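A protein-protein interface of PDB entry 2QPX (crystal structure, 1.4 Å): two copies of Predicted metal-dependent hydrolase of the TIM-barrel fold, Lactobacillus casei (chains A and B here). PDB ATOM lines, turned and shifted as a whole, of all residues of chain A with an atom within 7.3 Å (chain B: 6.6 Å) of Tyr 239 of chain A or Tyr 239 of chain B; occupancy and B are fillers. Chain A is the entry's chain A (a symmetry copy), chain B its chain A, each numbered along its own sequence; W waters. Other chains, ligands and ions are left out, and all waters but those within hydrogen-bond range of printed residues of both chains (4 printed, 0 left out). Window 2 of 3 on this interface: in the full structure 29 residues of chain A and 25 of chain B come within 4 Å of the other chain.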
ATOM      1  N   GLY A 175     -18.123 -23.550 -18.998  1.00  0.00           N
ATOM      2  CA  GLY A 175     -17.113 -22.573 -18.774  1.00  0.00           C
ATOM      3  C   GLY A 175     -16.168 -22.461 -19.966  1.00  0.00           C
ATOM      4  O   GLY A 175     -16.342 -23.142 -20.998  1.00  0.00           O
ATOM      5  N   LEU A 176     -15.164 -21.604 -19.814  1.00  0.00           N
ATOM      6  CA  LEU A 176     -14.303 -21.207 -20.921  1.00  0.00           C
ATOM      7  C   LEU A 176     -12.841 -21.665 -20.828  1.00  0.00           C
ATOM      8  O   LEU A 176     -12.007 -21.223 -21.613  1.00  0.00           O
ATOM      9  CB  LEU A 176     -14.344 -19.688 -21.151  1.00  0.00           C
ATOM     10  CG  LEU A 176     -15.687 -19.120 -21.628  1.00  0.00           C
ATOM     11  CD1 LEU A 176     -15.587 -17.589 -21.653  1.00  0.00           C
ATOM     12  CD2 LEU A 176     -16.018 -19.725 -22.994  1.00  0.00           C
ATOM     13  N   THR A 236     -25.170 -20.377 -14.592  1.00  0.00           N
ATOM     14  CA  THR A 236     -23.876 -20.159 -15.238  1.00  0.00           C
ATOM     15  C   THR A 236     -22.851 -19.986 -14.108  1.00  0.00           C
ATOM     16  O   THR A 236     -23.085 -19.276 -13.113  1.00  0.00           O
ATOM     17  CB  THR A 236     -23.888 -18.912 -16.107  1.00  0.00           C
ATOM     18  OG1 THR A 236     -24.888 -19.031 -17.155  1.00  0.00           O
ATOM     19  CG2 THR A 236     -22.517 -18.658 -16.746  1.00  0.00           C
ATOM     20  N   ASP A 237     -21.698 -20.611 -14.241  1.00  0.00           N
ATOM     21  CA  ASP A 237     -20.635 -20.379 -13.282  1.00  0.00           C
ATOM     22  C   ASP A 237     -19.778 -19.222 -13.822  1.00  0.00           C
ATOM     23  O   ASP A 237     -18.911 -19.440 -14.668  1.00  0.00           O
ATOM     24  CB  ASP A 237     -19.877 -21.671 -13.060  1.00  0.00           C
ATOM     25  CG  ASP A 237     -18.826 -21.552 -12.001  1.00  0.00           C
ATOM     26  OD1 ASP A 237     -18.580 -20.414 -11.536  1.00  0.00           O
ATOM     27  OD2 ASP A 237     -18.201 -22.612 -11.691  1.00  0.00           O
ATOM     28  N   MET A 238     -20.052 -17.995 -13.334  1.00  0.00           N
ATOM     29  CA  MET A 238     -19.406 -16.784 -13.876  1.00  0.00           C
ATOM     30  C   MET A 238     -17.906 -16.842 -13.566  1.00  0.00           C
ATOM     31  O   MET A 238     -17.098 -16.176 -14.263  1.00  0.00           O
ATOM     32  CB  MET A 238     -20.091 -15.469 -13.357  1.00  0.00           C
ATOM     33  CG  MET A 238     -19.422 -14.096 -13.774  1.00  0.00           C
ATOM     34  SD  MET A 238     -20.038 -12.432 -12.809  1.00  0.00           S
ATOM     35  CE  MET A 238     -21.544 -11.803 -13.917  1.00  0.00           C
ATOM     36  N   TYR A 239     -17.521 -17.633 -12.580  1.00  0.00           N
ATOM     37  CA  TYR A 239     -16.089 -17.756 -12.239  1.00  0.00           C
ATOM     38  C   TYR A 239     -15.281 -18.366 -13.365  1.00  0.00           C
ATOM     39  O   TYR A 239     -14.094 -18.051 -13.526  1.00  0.00           O
ATOM     40  CB  TYR A 239     -15.930 -18.544 -10.920  1.00  0.00           C
ATOM     41  CG  TYR A 239     -14.617 -18.416 -10.229  1.00  0.00           C
ATOM     42  CD1 TYR A 239     -14.367 -17.339  -9.381  1.00  0.00           C
ATOM     43  CD2 TYR A 239     -13.626 -19.386 -10.392  1.00  0.00           C
ATOM     44  CE1 TYR A 239     -13.141 -17.210  -8.732  1.00  0.00           C
ATOM     45  CE2 TYR A 239     -12.401 -19.279  -9.725  1.00  0.00           C
ATOM     46  CZ  TYR A 239     -12.171 -18.177  -8.901  1.00  0.00           C
ATOM     47  OH  TYR A 239     -10.945 -18.055  -8.258  1.00  0.00           O
ATOM     48  N   LEU A 240     -15.934 -19.222 -14.155  1.00  0.00           N
ATOM     49  CA  LEU A 240     -15.315 -19.905 -15.294  1.00  0.00           C
ATOM     50  C   LEU A 240     -15.508 -19.159 -16.591  1.00  0.00           C
ATOM     51  O   LEU A 240     -15.175 -19.664 -17.680  1.00  0.00           O
ATOM     52  CB  LEU A 240     -15.922 -21.321 -15.429  1.00  0.00           C
ATOM     53  CG  LEU A 240     -15.620 -22.226 -14.231  1.00  0.00           C
ATOM     54  CD1 LEU A 240     -16.190 -23.634 -14.492  1.00  0.00           C
ATOM     55  CD2 LEU A 240     -14.123 -22.294 -13.959  1.00  0.00           C
ATOM     56  N   GLY A 241     -16.096 -17.974 -16.516  1.00  0.00           N
ATOM     57  CA  GLY A 241     -16.391 -17.190 -17.708  1.00  0.00           C
ATOM     58  C   GLY A 241     -15.342 -16.146 -18.034  1.00  0.00           C
ATOM     59  O   GLY A 241     -15.610 -15.271 -18.863  1.00  0.00           O
ATOM     60  N   ASN A 242     -14.214 -16.168 -17.317  1.00  0.00           N
ATOM     61  CA  ASN A 242     -13.116 -15.226 -17.546  1.00  0.00           C
ATOM     62  C   ASN A 242     -12.438 -15.634 -18.873  1.00  0.00           C
ATOM     63  O   ASN A 242     -11.891 -16.735 -18.993  1.00  0.00           O
ATOM     64  CB  ASN A 242     -12.119 -15.270 -16.380  1.00  0.00           C
ATOM     65  CG  ASN A 242     -11.011 -14.231 -16.490  1.00  0.00           C
ATOM     66  OD1 ASN A 242     -10.597 -13.836 -17.593  1.00  0.00           O
ATOM     67  ND2 ASN A 242     -10.500 -13.789 -15.319  1.00  0.00           N
ATOM     68  N   LEU A 245      -9.178 -17.602 -19.674  1.00  0.00           N
ATOM     69  CA  LEU A 245      -9.151 -19.057 -19.634  1.00  0.00           C
ATOM     70  C   LEU A 245      -9.155 -19.675 -21.046  1.00  0.00           C
ATOM     71  O   LEU A 245      -8.799 -20.844 -21.220  1.00  0.00           O
ATOM     72  CB  LEU A 245     -10.309 -19.592 -18.799  1.00  0.00           C
ATOM     73  CG  LEU A 245     -10.310 -19.212 -17.310  1.00  0.00           C
ATOM     74  CD1 LEU A 245     -11.661 -19.530 -16.648  1.00  0.00           C
ATOM     75  CD2 LEU A 245      -9.144 -19.863 -16.599  1.00  0.00           C
ATOM     76  N   TYR A 268     -15.572  -9.002 -17.274  1.00  0.00           N
ATOM     77  CA  TYR A 268     -14.218  -9.295 -17.769  1.00  0.00           C
ATOM     78  C   TYR A 268     -13.906  -8.562 -19.070  1.00  0.00           C
ATOM     79  O   TYR A 268     -13.120  -9.015 -19.900  1.00  0.00           O
ATOM     80  CB  TYR A 268     -14.069 -10.782 -17.973  1.00  0.00           C
ATOM     81  CG  TYR A 268     -14.428 -11.636 -16.788  1.00  0.00           C
ATOM     82  CD1 TYR A 268     -13.644 -11.660 -15.658  1.00  0.00           C
ATOM     83  CD2 TYR A 268     -15.538 -12.464 -16.840  1.00  0.00           C
ATOM     84  CE1 TYR A 268     -13.963 -12.463 -14.575  1.00  0.00           C
ATOM     85  CE2 TYR A 268     -15.872 -13.297 -15.741  1.00  0.00           C
ATOM     86  CZ  TYR A 268     -15.084 -13.266 -14.620  1.00  0.00           C
ATOM     87  OH  TYR A 268     -15.397 -14.070 -13.535  1.00  0.00           O
ATOM     88  N   THR B 236      -5.995 -13.101   5.755  1.00  0.00           N
ATOM     89  CA  THR B 236      -7.158 -13.485   4.954  1.00  0.00           C
ATOM     90  C   THR B 236      -6.634 -13.773   3.540  1.00  0.00           C
ATOM     91  O   THR B 236      -5.813 -13.022   2.979  1.00  0.00           O
ATOM     92  CB  THR B 236      -8.189 -12.369   4.895  1.00  0.00           C
ATOM     93  OG1 THR B 236      -8.664 -12.043   6.229  1.00  0.00           O
ATOM     94  CG2 THR B 236      -9.385 -12.754   4.015  1.00  0.00           C
ATOM     95  N   ASP B 237      -7.100 -14.844   2.932  1.00  0.00           N
ATOM     96  CA  ASP B 237      -6.755 -15.099   1.547  1.00  0.00           C
ATOM     97  C   ASP B 237      -7.844 -14.446   0.678  1.00  0.00           C
ATOM     98  O   ASP B 237      -8.907 -15.033   0.478  1.00  0.00           O
ATOM     99  CB  ASP B 237      -6.599 -16.590   1.340  1.00  0.00           C
ATOM    100  CG  ASP B 237      -6.136 -16.939  -0.040  1.00  0.00           C
ATOM    101  OD1 ASP B 237      -6.078 -16.023  -0.895  1.00  0.00           O
ATOM    102  OD2 ASP B 237      -5.896 -18.163  -0.273  1.00  0.00           O
ATOM    103  N   MET B 238      -7.566 -13.220   0.190  1.00  0.00           N
ATOM    104  CA  MET B 238      -8.580 -12.425  -0.531  1.00  0.00           C
ATOM    105  C   MET B 238      -8.927 -13.139  -1.842  1.00  0.00           C
ATOM    106  O   MET B 238     -10.026 -12.906  -2.408  1.00  0.00           O
ATOM    107  CB  MET B 238      -8.119 -10.938  -0.743  1.00  0.00           C
ATOM    108  CG  MET B 238      -9.068 -10.007  -1.604  1.00  0.00           C
ATOM    109  SD  MET B 238      -8.320  -8.234  -2.216  1.00  0.00           S
ATOM    110  CE  MET B 238      -8.798  -7.013  -0.742  1.00  0.00           C
ATOM    111  N   TYR B 239      -8.049 -14.009  -2.310  1.00  0.00           N
ATOM    112  CA  TYR B 239      -8.327 -14.750  -3.558  1.00  0.00           C
ATOM    113  C   TYR B 239      -9.526 -15.666  -3.426  1.00  0.00           C
ATOM    114  O   TYR B 239     -10.236 -15.910  -4.411  1.00  0.00           O
ATOM    115  CB  TYR B 239      -7.061 -15.515  -4.005  1.00  0.00           C
ATOM    116  CG  TYR B 239      -7.035 -15.975  -5.421  1.00  0.00           C
ATOM    117  CD1 TYR B 239      -6.628 -15.112  -6.437  1.00  0.00           C
ATOM    118  CD2 TYR B 239      -7.385 -17.285  -5.754  1.00  0.00           C
ATOM    119  CE1 TYR B 239      -6.602 -15.533  -7.764  1.00  0.00           C
ATOM    120  CE2 TYR B 239      -7.338 -17.725  -7.081  1.00  0.00           C
ATOM    121  CZ  TYR B 239      -6.950 -16.831  -8.079  1.00  0.00           C
ATOM    122  OH  TYR B 239      -6.928 -17.259  -9.401  1.00  0.00           O
ATOM    123  N   LEU B 240      -9.759 -16.151  -2.205  1.00  0.00           N
ATOM    124  CA  LEU B 240     -10.874 -17.048  -1.891  1.00  0.00           C
ATOM    125  C   LEU B 240     -12.096 -16.306  -1.410  1.00  0.00           C
ATOM    126  O   LEU B 240     -13.085 -16.917  -0.962  1.00  0.00           O
ATOM    127  CB  LEU B 240     -10.428 -18.050  -0.800  1.00  0.00           C
ATOM    128  CG  LEU B 240      -9.305 -18.985  -1.258  1.00  0.00           C
ATOM    129  CD1 LEU B 240      -8.987 -19.997  -0.140  1.00  0.00           C
ATOM    130  CD2 LEU B 240      -9.682 -19.706  -2.546  1.00  0.00           C
ATOM    131  N   GLY B 241     -12.040 -14.983  -1.437  1.00  0.00           N
ATOM    132  CA  GLY B 241     -13.135 -14.160  -0.941  1.00  0.00           C
ATOM    133  C   GLY B 241     -14.092 -13.692  -2.019  1.00  0.00           C
ATOM    134  O   GLY B 241     -14.899 -12.796  -1.751  1.00  0.00           O
ATOM    135  N   ASN B 242     -13.932 -14.204  -3.243  1.00  0.00           N
ATOM    136  CA  ASN B 242     -14.802 -13.849  -4.366  1.00  0.00           C
ATOM    137  C   ASN B 242     -16.167 -14.527  -4.115  1.00  0.00           C
ATOM    138  O   ASN B 242     -16.264 -15.758  -4.067  1.00  0.00           O
ATOM    139  CB  ASN B 242     -14.187 -14.319  -5.692  1.00  0.00           C
ATOM    140  CG  ASN B 242     -14.977 -13.879  -6.917  1.00  0.00           C
ATOM    141  OD1 ASN B 242     -16.209 -13.718  -6.873  1.00  0.00           O
ATOM    142  ND2 ASN B 242     -14.259 -13.698  -8.047  1.00  0.00           N
ATOM    143  N   LEU B 244     -18.653 -15.183  -5.928  1.00  0.00           N
ATOM    144  CA  LEU B 244     -19.078 -16.161  -6.936  1.00  0.00           C
ATOM    145  C   LEU B 244     -18.797 -17.588  -6.449  1.00  0.00           C
ATOM    146  O   LEU B 244     -19.487 -18.522  -6.861  1.00  0.00           O
ATOM    147  CB  LEU B 244     -18.378 -15.926  -8.269  1.00  0.00           C
ATOM    148  CG  LEU B 244     -18.603 -14.588  -8.980  1.00  0.00           C
ATOM    149  CD1 LEU B 244     -17.812 -14.502 -10.286  1.00  0.00           C
ATOM    150  CD2 LEU B 244     -20.118 -14.334  -9.182  1.00  0.00           C
ATOM    151  N   LEU B 245     -17.820 -17.743  -5.555  1.00  0.00           N
ATOM    152  CA  LEU B 245     -17.479 -19.059  -5.034  1.00  0.00           C
ATOM    153  C   LEU B 245     -18.585 -19.624  -4.123  1.00  0.00           C
ATOM    154  O   LEU B 245     -18.634 -20.832  -3.870  1.00  0.00           O
ATOM    155  CB  LEU B 245     -16.139 -19.017  -4.308  1.00  0.00           C
ATOM    156  CG  LEU B 245     -14.911 -18.662  -5.160  1.00  0.00           C
ATOM    157  CD1 LEU B 245     -13.689 -18.343  -4.283  1.00  0.00           C
ATOM    158  CD2 LEU B 245     -14.636 -19.756  -6.169  1.00  0.00           C
ATOM    159  N   TYR B 268     -14.882  -7.178  -4.954  1.00  0.00           N
ATOM    160  CA  TYR B 268     -15.824  -8.045  -5.677  1.00  0.00           C
ATOM    161  C   TYR B 268     -17.261  -7.539  -5.590  1.00  0.00           C
ATOM    162  O   TYR B 268     -18.224  -8.301  -5.642  1.00  0.00           O
ATOM    163  CB  TYR B 268     -15.743  -9.446  -5.124  1.00  0.00           C
ATOM    164  CG  TYR B 268     -14.363 -10.042  -5.074  1.00  0.00           C
ATOM    165  CD1 TYR B 268     -13.694 -10.400  -6.220  1.00  0.00           C
ATOM    166  CD2 TYR B 268     -13.760 -10.293  -3.851  1.00  0.00           C
ATOM    167  CE1 TYR B 268     -12.431 -10.969  -6.172  1.00  0.00           C
ATOM    168  CE2 TYR B 268     -12.471 -10.882  -3.787  1.00  0.00           C
ATOM    169  CZ  TYR B 268     -11.823 -11.192  -4.955  1.00  0.00           C
ATOM    170  OH  TYR B 268     -10.561 -11.764  -4.912  1.00  0.00           O
HETATM  171  O   HOH W   1     -19.928 -18.972  -9.670  1.00  0.00           O
HETATM  172  O   HOH W   2      -8.866 -19.395  -9.798  1.00  0.00           O
HETATM  173  O   HOH W   3     -14.834 -12.528 -10.768  1.00  0.00           O
HETATM  174  O   HOH W   4     -10.796 -15.567  -7.020  1.00  0.00           O
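OD1 of Asp 237 of chain B lies close to N of Tyr 239 of chain B (3.2 Å).
N of Leu 244 of chain B lies within hydrogen-bond range of OD1 of Asn 242 of chain B.
OD1 of Asp 237 of chain A lies close to N of Tyr 239 of chain A.
The backbone carbonyl oxygen (O) of Met 238 of chain A lies within hydrogen-bond range of the side-chain hydroxyl (OH) of Tyr 268 of chain A (2.8 Å).
CG of Met 238 of chain A touches CD1 of Leu 244 of chain B (3.9 Å).
CE2 of Tyr 239 of chain B touches OH of Tyr 239 of chain A, 3.8 Å away.
Tyr 239 of chain A touches Asn 242 of chain B.
Leu 244 of chain B touches Tyr 239 of chain A (CD1 to N, 3.9 Å).
Leu 245 of chain B touches Tyr 239 of chain A (CD2 to CE1, 3.9 Å).
Tyr 239 of chain A touches four residues of chain B.
Printed residues of chain A within 4 Å of Tyr 239 of chain B: Tyr 239.
Of the printed residues of chain A, Leu 244 of chain B touches Met 238 and Tyr 239.
Printed residues of chain A within 4 Å of Leu 245 of chain B: Tyr 239 (3.9 Å).
Of the printed residues of chain B, Met 238 of chain A touches Leu 244 (3.9 Å).
Printed residues of chain A within 4 Å of Asn 242 of chain B: Tyr 239.
Tyr 268 of chain A touches none of the printed residues of chain B.
The nearest printed residue of chain B that does not touch Tyr 239 of chain A is Leu 240 of chain B (6.1 Å).
The nearest printed residue of chain A that does not touch Leu 245 of chain B is Asp 237 of chain A (6.6 Å).
Hydrophobic or aromatic side chains of chain A that line the printed part of chain B: Met 238 and Tyr 239.
Among the printed residues, 5 pairs touch across the chains.
Tyr 239 of chain B touches its own counterpart, Tyr 239 of chain A.
Tyr 239 of chain A touches Asn 242 of chain B, but with the chains exchanged Asn 242 of chain A does not touch Tyr 239 of chain B (7.7 Å).
Tyr 239 of chain A touches Leu 245 of chain B, but with the chains exchanged Leu 245 of chain A does not touch Tyr 239 of chain B (8.0 Å).
Of the 5 pairs that touch across the chains among the printed residues, 1 has its exchanged pair printed and touching as well.
Water W4 bridges O of Tyr 239 of chain B (2.7 Å) and OH of Tyr 239 of chain A (2.8 Å).
Water W1 bridges OD1 of Asp 237 of chain A (2.7 Å) and O of Leu 244 of chain B (2.9 Å).
Water W2 bridges the side-chain hydroxyl of Tyr 239 of chain B and the side-chain hydroxyl of Tyr 239 of chain A.
Water W3 lies within hydrogen-bond range of ND2 of Asn 242 of chain B and OH of Tyr 268 of chain A.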
